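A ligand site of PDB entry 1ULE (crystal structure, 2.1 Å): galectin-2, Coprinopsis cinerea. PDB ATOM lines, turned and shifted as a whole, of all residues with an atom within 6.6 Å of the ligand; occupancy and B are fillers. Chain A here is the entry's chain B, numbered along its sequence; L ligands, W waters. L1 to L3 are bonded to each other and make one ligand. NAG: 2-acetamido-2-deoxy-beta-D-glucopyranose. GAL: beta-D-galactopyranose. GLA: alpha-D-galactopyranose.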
ATOM      1  N   THR A  36     -19.531 -16.302   1.019  1.00  0.00           N
ATOM      2  CA  THR A  36     -19.818 -15.569   2.236  1.00  0.00           C
ATOM      3  C   THR A  36     -20.739 -16.362   3.161  1.00  0.00           C
ATOM      4  O   THR A  36     -21.828 -16.777   2.777  1.00  0.00           O
ATOM      5  CB  THR A  36     -20.440 -14.211   1.902  1.00  0.00           C
ATOM      6  OG1 THR A  36     -19.448 -13.398   1.245  1.00  0.00           O
ATOM      7  CG2 THR A  36     -20.915 -13.491   3.162  1.00  0.00           C
ATOM      8  N   VAL A  38     -22.588 -16.467   7.035  1.00  0.00           N
ATOM      9  CA  VAL A  38     -23.007 -15.595   8.124  1.00  0.00           C
ATOM     10  C   VAL A  38     -23.609 -16.270   9.350  1.00  0.00           C
ATOM     11  O   VAL A  38     -24.361 -17.246   9.233  1.00  0.00           O
ATOM     12  CB  VAL A  38     -24.043 -14.563   7.595  1.00  0.00           C
ATOM     13  CG1 VAL A  38     -24.752 -13.870   8.754  1.00  0.00           C
ATOM     14  CG2 VAL A  38     -23.328 -13.533   6.733  1.00  0.00           C
ATOM     15  N   ASN A  40     -25.588 -15.064  12.970  1.00  0.00           N
ATOM     16  CA  ASN A  40     -26.205 -13.964  13.717  1.00  0.00           C
ATOM     17  C   ASN A  40     -26.739 -14.403  15.075  1.00  0.00           C
ATOM     18  O   ASN A  40     -27.338 -15.473  15.203  1.00  0.00           O
ATOM     19  CB  ASN A  40     -27.410 -13.373  12.956  1.00  0.00           C
ATOM     20  CG  ASN A  40     -27.019 -12.639  11.688  1.00  0.00           C
ATOM     21  OD1 ASN A  40     -25.993 -11.965  11.638  1.00  0.00           O
ATOM     22  ND2 ASN A  40     -27.866 -12.730  10.666  1.00  0.00           N
ATOM     23  N   ILE A  48     -30.379  -7.875  15.551  1.00  0.00           N
ATOM     24  CA  ILE A  48     -29.128  -8.586  15.328  1.00  0.00           C
ATOM     25  C   ILE A  48     -28.072  -8.024  16.266  1.00  0.00           C
ATOM     26  O   ILE A  48     -27.408  -7.028  15.964  1.00  0.00           O
ATOM     27  CB  ILE A  48     -28.682  -8.448  13.857  1.00  0.00           C
ATOM     28  CG1 ILE A  48     -29.789  -8.981  12.939  1.00  0.00           C
ATOM     29  CG2 ILE A  48     -27.385  -9.216  13.628  1.00  0.00           C
ATOM     30  CD1 ILE A  48     -29.467  -8.869  11.469  1.00  0.00           C
ATOM     31  N   HIS A  51     -23.388  -9.766  14.433  1.00  0.00           N
ATOM     32  CA  HIS A  51     -23.396 -10.214  13.047  1.00  0.00           C
ATOM     33  C   HIS A  51     -21.974 -10.587  12.697  1.00  0.00           C
ATOM     34  O   HIS A  51     -21.059  -9.768  12.846  1.00  0.00           O
ATOM     35  CB  HIS A  51     -23.879  -9.068  12.141  1.00  0.00           C
ATOM     36  CG  HIS A  51     -23.812  -9.363  10.678  1.00  0.00           C
ATOM     37  ND1 HIS A  51     -24.665 -10.250  10.048  1.00  0.00           N
ATOM     38  CD2 HIS A  51     -23.032  -8.837   9.699  1.00  0.00           C
ATOM     39  CE1 HIS A  51     -24.416 -10.247   8.750  1.00  0.00           C
ATOM     40  NE2 HIS A  51     -23.430  -9.403   8.505  1.00  0.00           N
ATOM     41  N   SER A  53     -19.907 -11.868   9.536  1.00  0.00           N
ATOM     42  CA  SER A  53     -19.928 -12.108   8.096  1.00  0.00           C
ATOM     43  C   SER A  53     -18.540 -12.499   7.602  1.00  0.00           C
ATOM     44  O   SER A  53     -17.682 -11.653   7.404  1.00  0.00           O
ATOM     45  CB  SER A  53     -20.410 -10.846   7.364  1.00  0.00           C
ATOM     46  OG  SER A  53     -20.401 -11.043   5.961  1.00  0.00           O
ATOM     47  N   ARG A  55     -16.112 -13.483   4.879  1.00  0.00           N
ATOM     48  CA  ARG A  55     -16.008 -13.291   3.434  1.00  0.00           C
ATOM     49  C   ARG A  55     -14.662 -13.712   2.839  1.00  0.00           C
ATOM     50  O   ARG A  55     -13.700 -12.934   2.816  1.00  0.00           O
ATOM     51  CB  ARG A  55     -16.272 -11.815   3.089  1.00  0.00           C
ATOM     52  CG  ARG A  55     -17.581 -11.283   3.640  1.00  0.00           C
ATOM     53  CD  ARG A  55     -17.664  -9.767   3.501  1.00  0.00           C
ATOM     54  NE  ARG A  55     -18.904  -9.230   4.068  1.00  0.00           N
ATOM     55  CZ  ARG A  55     -19.204  -7.938   4.105  1.00  0.00           C
ATOM     56  NH1 ARG A  55     -18.365  -7.053   3.604  1.00  0.00           N
ATOM     57  NH2 ARG A  55     -20.352  -7.539   4.643  1.00  0.00           N
ATOM     58  N   GLU A  58     -13.558 -11.520  -0.256  1.00  0.00           N
ATOM     59  CA  GLU A  58     -13.092 -10.190   0.100  1.00  0.00           C
ATOM     60  C   GLU A  58     -11.937 -10.295   1.084  1.00  0.00           C
ATOM     61  O   GLU A  58     -11.277  -9.298   1.401  1.00  0.00           O
ATOM     62  CB  GLU A  58     -14.252  -9.402   0.717  1.00  0.00           C
ATOM     63  CG  GLU A  58     -14.071  -7.895   0.730  1.00  0.00           C
ATOM     64  CD  GLU A  58     -15.275  -7.176   1.323  1.00  0.00           C
ATOM     65  OE1 GLU A  58     -16.408  -7.645   1.095  1.00  0.00           O
ATOM     66  OE2 GLU A  58     -15.080  -6.144   1.993  1.00  0.00           O
ATOM     67  N   VAL A  62     -16.389  -9.526   8.861  1.00  0.00           N
ATOM     68  CA  VAL A  62     -16.997  -8.288   9.311  1.00  0.00           C
ATOM     69  C   VAL A  62     -17.957  -8.481  10.473  1.00  0.00           C
ATOM     70  O   VAL A  62     -18.813  -9.371  10.443  1.00  0.00           O
ATOM     71  CB  VAL A  62     -17.769  -7.615   8.145  1.00  0.00           C
ATOM     72  CG1 VAL A  62     -18.370  -6.284   8.612  1.00  0.00           C
ATOM     73  CG2 VAL A  62     -16.824  -7.392   6.967  1.00  0.00           C
ATOM     74  N   PHE A  63     -17.817  -7.654  11.506  1.00  0.00           N
ATOM     75  CA  PHE A  63     -18.685  -7.714  12.676  1.00  0.00           C
ATOM     76  C   PHE A  63     -19.545  -6.455  12.721  1.00  0.00           C
ATOM     77  O   PHE A  63     -19.035  -5.355  12.517  1.00  0.00           O
ATOM     78  CB  PHE A  63     -17.859  -7.828  13.953  1.00  0.00           C
ATOM     79  CG  PHE A  63     -16.907  -8.996  13.975  1.00  0.00           C
ATOM     80  CD1 PHE A  63     -15.685  -8.923  13.318  1.00  0.00           C
ATOM     81  CD2 PHE A  63     -17.237 -10.161  14.646  1.00  0.00           C
ATOM     82  CE1 PHE A  63     -14.796 -10.012  13.342  1.00  0.00           C
ATOM     83  CE2 PHE A  63     -16.358 -11.249  14.668  1.00  0.00           C
ATOM     84  CZ  PHE A  63     -15.136 -11.166  14.010  1.00  0.00           C
ATOM     85  N   ASN A  64     -20.829  -6.619  12.988  1.00  0.00           N
ATOM     86  CA  ASN A  64     -21.724  -5.475  13.057  1.00  0.00           C
ATOM     87  C   ASN A  64     -22.981  -5.817  13.865  1.00  0.00           C
ATOM     88  O   ASN A  64     -23.123  -6.928  14.363  1.00  0.00           O
ATOM     89  CB  ASN A  64     -22.125  -5.047  11.633  1.00  0.00           C
ATOM     90  CG  ASN A  64     -22.344  -3.542  11.512  1.00  0.00           C
ATOM     91  OD1 ASN A  64     -22.736  -2.877  12.464  1.00  0.00           O
ATOM     92  ND2 ASN A  64     -22.093  -3.006  10.312  1.00  0.00           N
ATOM     93  N   SER A  65     -23.882  -4.844  14.011  1.00  0.00           N
ATOM     94  CA  SER A  65     -25.133  -5.015  14.742  1.00  0.00           C
ATOM     95  C   SER A  65     -26.207  -4.177  14.036  1.00  0.00           C
ATOM     96  O   SER A  65     -25.884  -3.208  13.345  1.00  0.00           O
ATOM     97  CB  SER A  65     -24.998  -4.543  16.187  1.00  0.00           C
ATOM     98  OG  SER A  65     -24.003  -5.270  16.897  1.00  0.00           O
ATOM     99  N   ARG A  66     -27.463  -4.538  14.236  1.00  0.00           N
ATOM    100  CA  ARG A  66     -28.569  -3.828  13.599  1.00  0.00           C
ATOM    101  C   ARG A  66     -29.891  -4.207  14.243  1.00  0.00           C
ATOM    102  O   ARG A  66     -30.094  -5.346  14.638  1.00  0.00           O
ATOM    103  CB  ARG A  66     -28.599  -4.206  12.119  1.00  0.00           C
ATOM    104  CG  ARG A  66     -29.725  -3.590  11.311  1.00  0.00           C
ATOM    105  CD  ARG A  66     -29.950  -4.375  10.018  1.00  0.00           C
ATOM    106  NE  ARG A  66     -31.002  -5.376  10.179  1.00  0.00           N
ATOM    107  CZ  ARG A  66     -31.234  -6.378   9.337  1.00  0.00           C
ATOM    108  NH1 ARG A  66     -30.479  -6.515   8.257  1.00  0.00           N
ATOM    109  NH2 ARG A  66     -32.220  -7.234   9.573  1.00  0.00           N
ATOM    110  N   TRP A  72     -27.410  -0.970   9.273  1.00  0.00           N
ATOM    111  CA  TRP A  72     -26.186  -1.488   9.852  1.00  0.00           C
ATOM    112  C   TRP A  72     -25.406  -0.308  10.407  1.00  0.00           C
ATOM    113  O   TRP A  72     -25.604   0.823   9.982  1.00  0.00           O
ATOM    114  CB  TRP A  72     -25.359  -2.202   8.780  1.00  0.00           C
ATOM    115  CG  TRP A  72     -25.936  -3.507   8.368  1.00  0.00           C
ATOM    116  CD1 TRP A  72     -26.593  -3.794   7.204  1.00  0.00           C
ATOM    117  CD2 TRP A  72     -25.960  -4.714   9.139  1.00  0.00           C
ATOM    118  NE1 TRP A  72     -27.028  -5.096   7.203  1.00  0.00           N
ATOM    119  CE2 TRP A  72     -26.644  -5.691   8.378  1.00  0.00           C
ATOM    120  CE3 TRP A  72     -25.460  -5.066  10.398  1.00  0.00           C
ATOM    121  CZ2 TRP A  72     -26.853  -7.003   8.840  1.00  0.00           C
ATOM    122  CZ3 TRP A  72     -25.668  -6.368  10.859  1.00  0.00           C
ATOM    123  CH2 TRP A  72     -26.348  -7.317  10.084  1.00  0.00           C
ATOM    124  N   GLY A  73     -24.528  -0.575  11.377  1.00  0.00           N
ATOM    125  CA  GLY A  73     -23.741   0.495  11.951  1.00  0.00           C
ATOM    126  C   GLY A  73     -22.333   0.440  11.406  1.00  0.00           C
ATOM    127  O   GLY A  73     -22.109  -0.187  10.369  1.00  0.00           O
ATOM    128  N   PRO A  74     -21.356   1.082  12.058  1.00  0.00           N
ATOM    129  CA  PRO A  74     -19.992   1.026  11.539  1.00  0.00           C
ATOM    130  C   PRO A  74     -19.499  -0.415  11.618  1.00  0.00           C
ATOM    131  O   PRO A  74     -19.886  -1.164  12.511  1.00  0.00           O
ATOM    132  CB  PRO A  74     -19.225   1.951  12.490  1.00  0.00           C
ATOM    133  CG  PRO A  74     -19.998   1.854  13.768  1.00  0.00           C
ATOM    134  CD  PRO A  74     -21.422   1.901  13.285  1.00  0.00           C
ATOM    135  N   GLU A  75     -18.673  -0.807  10.658  1.00  0.00           N
ATOM    136  CA  GLU A  75     -18.157  -2.167  10.614  1.00  0.00           C
ATOM    137  C   GLU A  75     -16.831  -2.312  11.327  1.00  0.00           C
ATOM    138  O   GLU A  75     -15.988  -1.420  11.293  1.00  0.00           O
ATOM    139  CB  GLU A  75     -17.958  -2.637   9.172  1.00  0.00           C
ATOM    140  CG  GLU A  75     -19.156  -2.467   8.255  1.00  0.00           C
ATOM    141  CD  GLU A  75     -18.929  -3.140   6.910  1.00  0.00           C
ATOM    142  OE1 GLU A  75     -17.783  -3.104   6.425  1.00  0.00           O
ATOM    143  OE2 GLU A  75     -19.888  -3.701   6.339  1.00  0.00           O
ATOM    144  N   ARG A  77     -13.798  -4.897  11.215  1.00  0.00           N
ATOM    145  CA  ARG A  77     -13.338  -6.017  10.414  1.00  0.00           C
ATOM    146  C   ARG A  77     -11.885  -6.436  10.603  1.00  0.00           C
ATOM    147  O   ARG A  77     -11.032  -5.634  11.003  1.00  0.00           O
ATOM    148  CB  ARG A  77     -13.582  -5.718   8.925  1.00  0.00           C
ATOM    149  CG  ARG A  77     -13.085  -4.359   8.465  1.00  0.00           C
ATOM    150  CD  ARG A  77     -13.178  -4.206   6.944  1.00  0.00           C
ATOM    151  NE  ARG A  77     -14.557  -4.103   6.456  1.00  0.00           N
ATOM    152  CZ  ARG A  77     -14.903  -4.339   5.195  1.00  0.00           C
ATOM    153  NH1 ARG A  77     -13.989  -4.692   4.299  1.00  0.00           N
ATOM    154  NH2 ARG A  77     -16.172  -4.224   4.819  1.00  0.00           N
ATOM    155  N   ASN A 126     -26.567 -18.317   7.919  1.00  0.00           N
ATOM    156  CA  ASN A 126     -26.941 -18.080   6.528  1.00  0.00           C
ATOM    157  C   ASN A 126     -25.779 -18.180   5.547  1.00  0.00           C
ATOM    158  O   ASN A 126     -24.678 -17.680   5.817  1.00  0.00           O
ATOM    159  CB  ASN A 126     -27.602 -16.703   6.361  1.00  0.00           C
ATOM    160  CG  ASN A 126     -28.807 -16.519   7.263  1.00  0.00           C
ATOM    161  OD1 ASN A 126     -29.689 -17.373   7.316  1.00  0.00           O
ATOM    162  ND2 ASN A 126     -28.849 -15.393   7.964  1.00  0.00           N
HETATM  163  C1  NAG L   1     -20.398  -1.540   1.592  1.00  0.00           C
HETATM  164  C2  NAG L   1     -19.624  -2.275   2.687  1.00  0.00           C
HETATM  165  C3  NAG L   1     -20.198  -3.681   2.831  1.00  0.00           C
HETATM  166  C4  NAG L   1     -21.704  -3.613   3.119  1.00  0.00           C
HETATM  167  C5  NAG L   1     -22.409  -2.750   2.052  1.00  0.00           C
HETATM  168  C6  NAG L   1     -23.871  -2.509   2.368  1.00  0.00           C
HETATM  169  C7  NAG L   1     -17.328  -1.583   2.951  1.00  0.00           C
HETATM  170  C8  NAG L   1     -15.862  -1.807   2.612  1.00  0.00           C
HETATM  171  N2  NAG L   1     -18.221  -2.352   2.328  1.00  0.00           N
HETATM  172  O1  NAG L   1     -19.919  -0.252   1.467  1.00  0.00           O
HETATM  173  O3  NAG L   1     -19.535  -4.368   3.886  1.00  0.00           O
HETATM  174  O4  NAG L   1     -22.251  -4.935   3.100  1.00  0.00           O
HETATM  175  O5  NAG L   1     -21.781  -1.453   1.962  1.00  0.00           O
HETATM  176  O6  NAG L   1     -24.031  -1.877   3.625  1.00  0.00           O
HETATM  177  O7  NAG L   1     -17.635  -0.722   3.779  1.00  0.00           O
HETATM  178  C1  GAL L   2     -23.161  -5.240   4.091  1.00  0.00           C
HETATM  179  C2  GAL L   2     -23.862  -6.559   3.760  1.00  0.00           C
HETATM  180  C3  GAL L   2     -24.728  -7.029   4.914  1.00  0.00           C
HETATM  181  C4  GAL L   2     -23.937  -7.043   6.222  1.00  0.00           C
HETATM  182  C5  GAL L   2     -23.309  -5.670   6.445  1.00  0.00           C
HETATM  183  C6  GAL L   2     -22.483  -5.592   7.711  1.00  0.00           C
HETATM  184  O2  GAL L   2     -24.675  -6.378   2.606  1.00  0.00           O
HETATM  185  O3  GAL L   2     -25.212  -8.357   4.628  1.00  0.00           O
HETATM  186  O4  GAL L   2     -22.914  -8.030   6.151  1.00  0.00           O
HETATM  187  O5  GAL L   2     -22.443  -5.346   5.334  1.00  0.00           O
HETATM  188  O6  GAL L   2     -21.760  -4.366   7.775  1.00  0.00           O
HETATM  189  C1  GLA L   3     -26.308  -8.777   5.383  1.00  0.00           C
HETATM  190  C2  GLA L   3     -26.738 -10.177   4.930  1.00  0.00           C
HETATM  191  C3  GLA L   3     -27.374 -10.123   3.541  1.00  0.00           C
HETATM  192  C4  GLA L   3     -28.500  -9.078   3.510  1.00  0.00           C
HETATM  193  C5  GLA L   3     -27.955  -7.729   3.983  1.00  0.00           C
HETATM  194  C6  GLA L   3     -29.021  -6.654   4.065  1.00  0.00           C
HETATM  195  O2  GLA L   3     -25.607 -11.038   4.902  1.00  0.00           O
HETATM  196  O3  GLA L   3     -27.908 -11.401   3.210  1.00  0.00           O
HETATM  197  O4  GLA L   3     -29.566  -9.487   4.359  1.00  0.00           O
HETATM  198  O5  GLA L   3     -27.402  -7.875   5.307  1.00  0.00           O
HETATM  199  O6  GLA L   3     -28.442  -5.409   4.416  1.00  0.00           O
HETATM  200  O   HOH W   1     -22.840 -10.460   4.776  1.00  0.00           O
HETATM  201  O   HOH W   2     -23.449   0.800   3.065  1.00  0.00           O
HETATM  202  O   HOH W   3     -29.531  -9.040   7.356  1.00  0.00           O
HETATM  203  O   HOH W   4     -17.609  -4.844   0.969  1.00  0.00           O
HETATM  204  O   HOH W   5     -16.059  -0.613   6.137  1.00  0.00           O
HETATM  205  O   HOH W   6     -26.627  -1.522   3.875  1.00  0.00           O
HETATM  206  O   HOH W   7     -27.427 -13.043   6.548  1.00  0.00           O
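The side-chain carboxylate (OE2) of Glu 75 is in hydrogen-bond range of an oxygen (O6) of GAL L2 (2.5 Å). O4 of GAL L2 lies within hydrogen-bond range of NE2 of His 51 (2.8 Å). NH1 of Arg 55 sits at hydrogen-bond distance from O3 of NAG L1, at 2.9 Å. ND2 of Asn 64 is in hydrogen-bond range of O6 of GAL L2, at 2.9 Å. O6 of GLA L3 is in hydrogen-bond range of NE1 of Trp 72, 3.1 Å away. The guanidinium group of Arg 77 lies close to an oxygen (O3) of NAG L1, 3.5 Å away.
The backbone NH (N) of Ser 53 lies within hydrogen-bond range of the backbone carbonyl oxygen (O) of Val 62, at 2.9 Å. The side-chain amide nitrogen (ND2) of Asn 64 lies within hydrogen-bond range of the backbone carbonyl oxygen (O) of Gly 73, 2.8 Å away. ND1 of His 51 is in hydrogen-bond range of OD1 of Asn 40 (2.7 Å). The side-chain carboxylate (OE1) of Glu 58 is in salt-bridge range of the guanidinium group (NH1) of Arg 55, at 3.2 Å. The side-chain amide oxygen (OD1) of Asn 64 sits close to the backbone carbonyl oxygen (O) of Pro 74, 3.3 Å away. NE of Arg 55 is in hydrogen-bond range of OG of Ser 53, 3.0 Å away. The backbone carbonyl oxygen (O) of Asn 126 lies within hydrogen-bond range of the backbone NH (N) of Val 38, at 2.7 Å. The backbone NH (N) of His 51 lies within hydrogen-bond range of the backbone carbonyl oxygen (O) of Asn 64.
CG2 of Val 38 touches O2 of GLA L3, 3.8 Å away. OG of Ser 53 touches O4 of GAL L2, at 3.9 Å. CG1 of Val 62 touches O6 of GAL L2 (3.98 Å). The nearest printed residue that does not touch the ligand is Arg 66 (4.4 Å).
Water W1 lies within hydrogen-bond range of OG of Ser 53 (2.8 Å) and O4 of GAL L2 (2.8 Å). Water W5 lies within hydrogen-bond range of an oxygen (O7) of NAG L1 (2.8 Å) and the side-chain carboxylate (OE1) of Glu 75 (3.0 Å). Water W4 lies within hydrogen-bond range of a nitrogen (N2) of NAG L1 (2.9 Å) and the side-chain carboxylate (OE2) of Glu 58 (3.0 Å). Water W3 bridges NH1 of Arg 66 (2.8 Å) and O4 of GLA L3 (3.0 Å). Water W7 bridges the side-chain amide nitrogen of Asn 126 (3.1 Å) and an oxygen (O2) of GLA L3 (3.2 Å).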
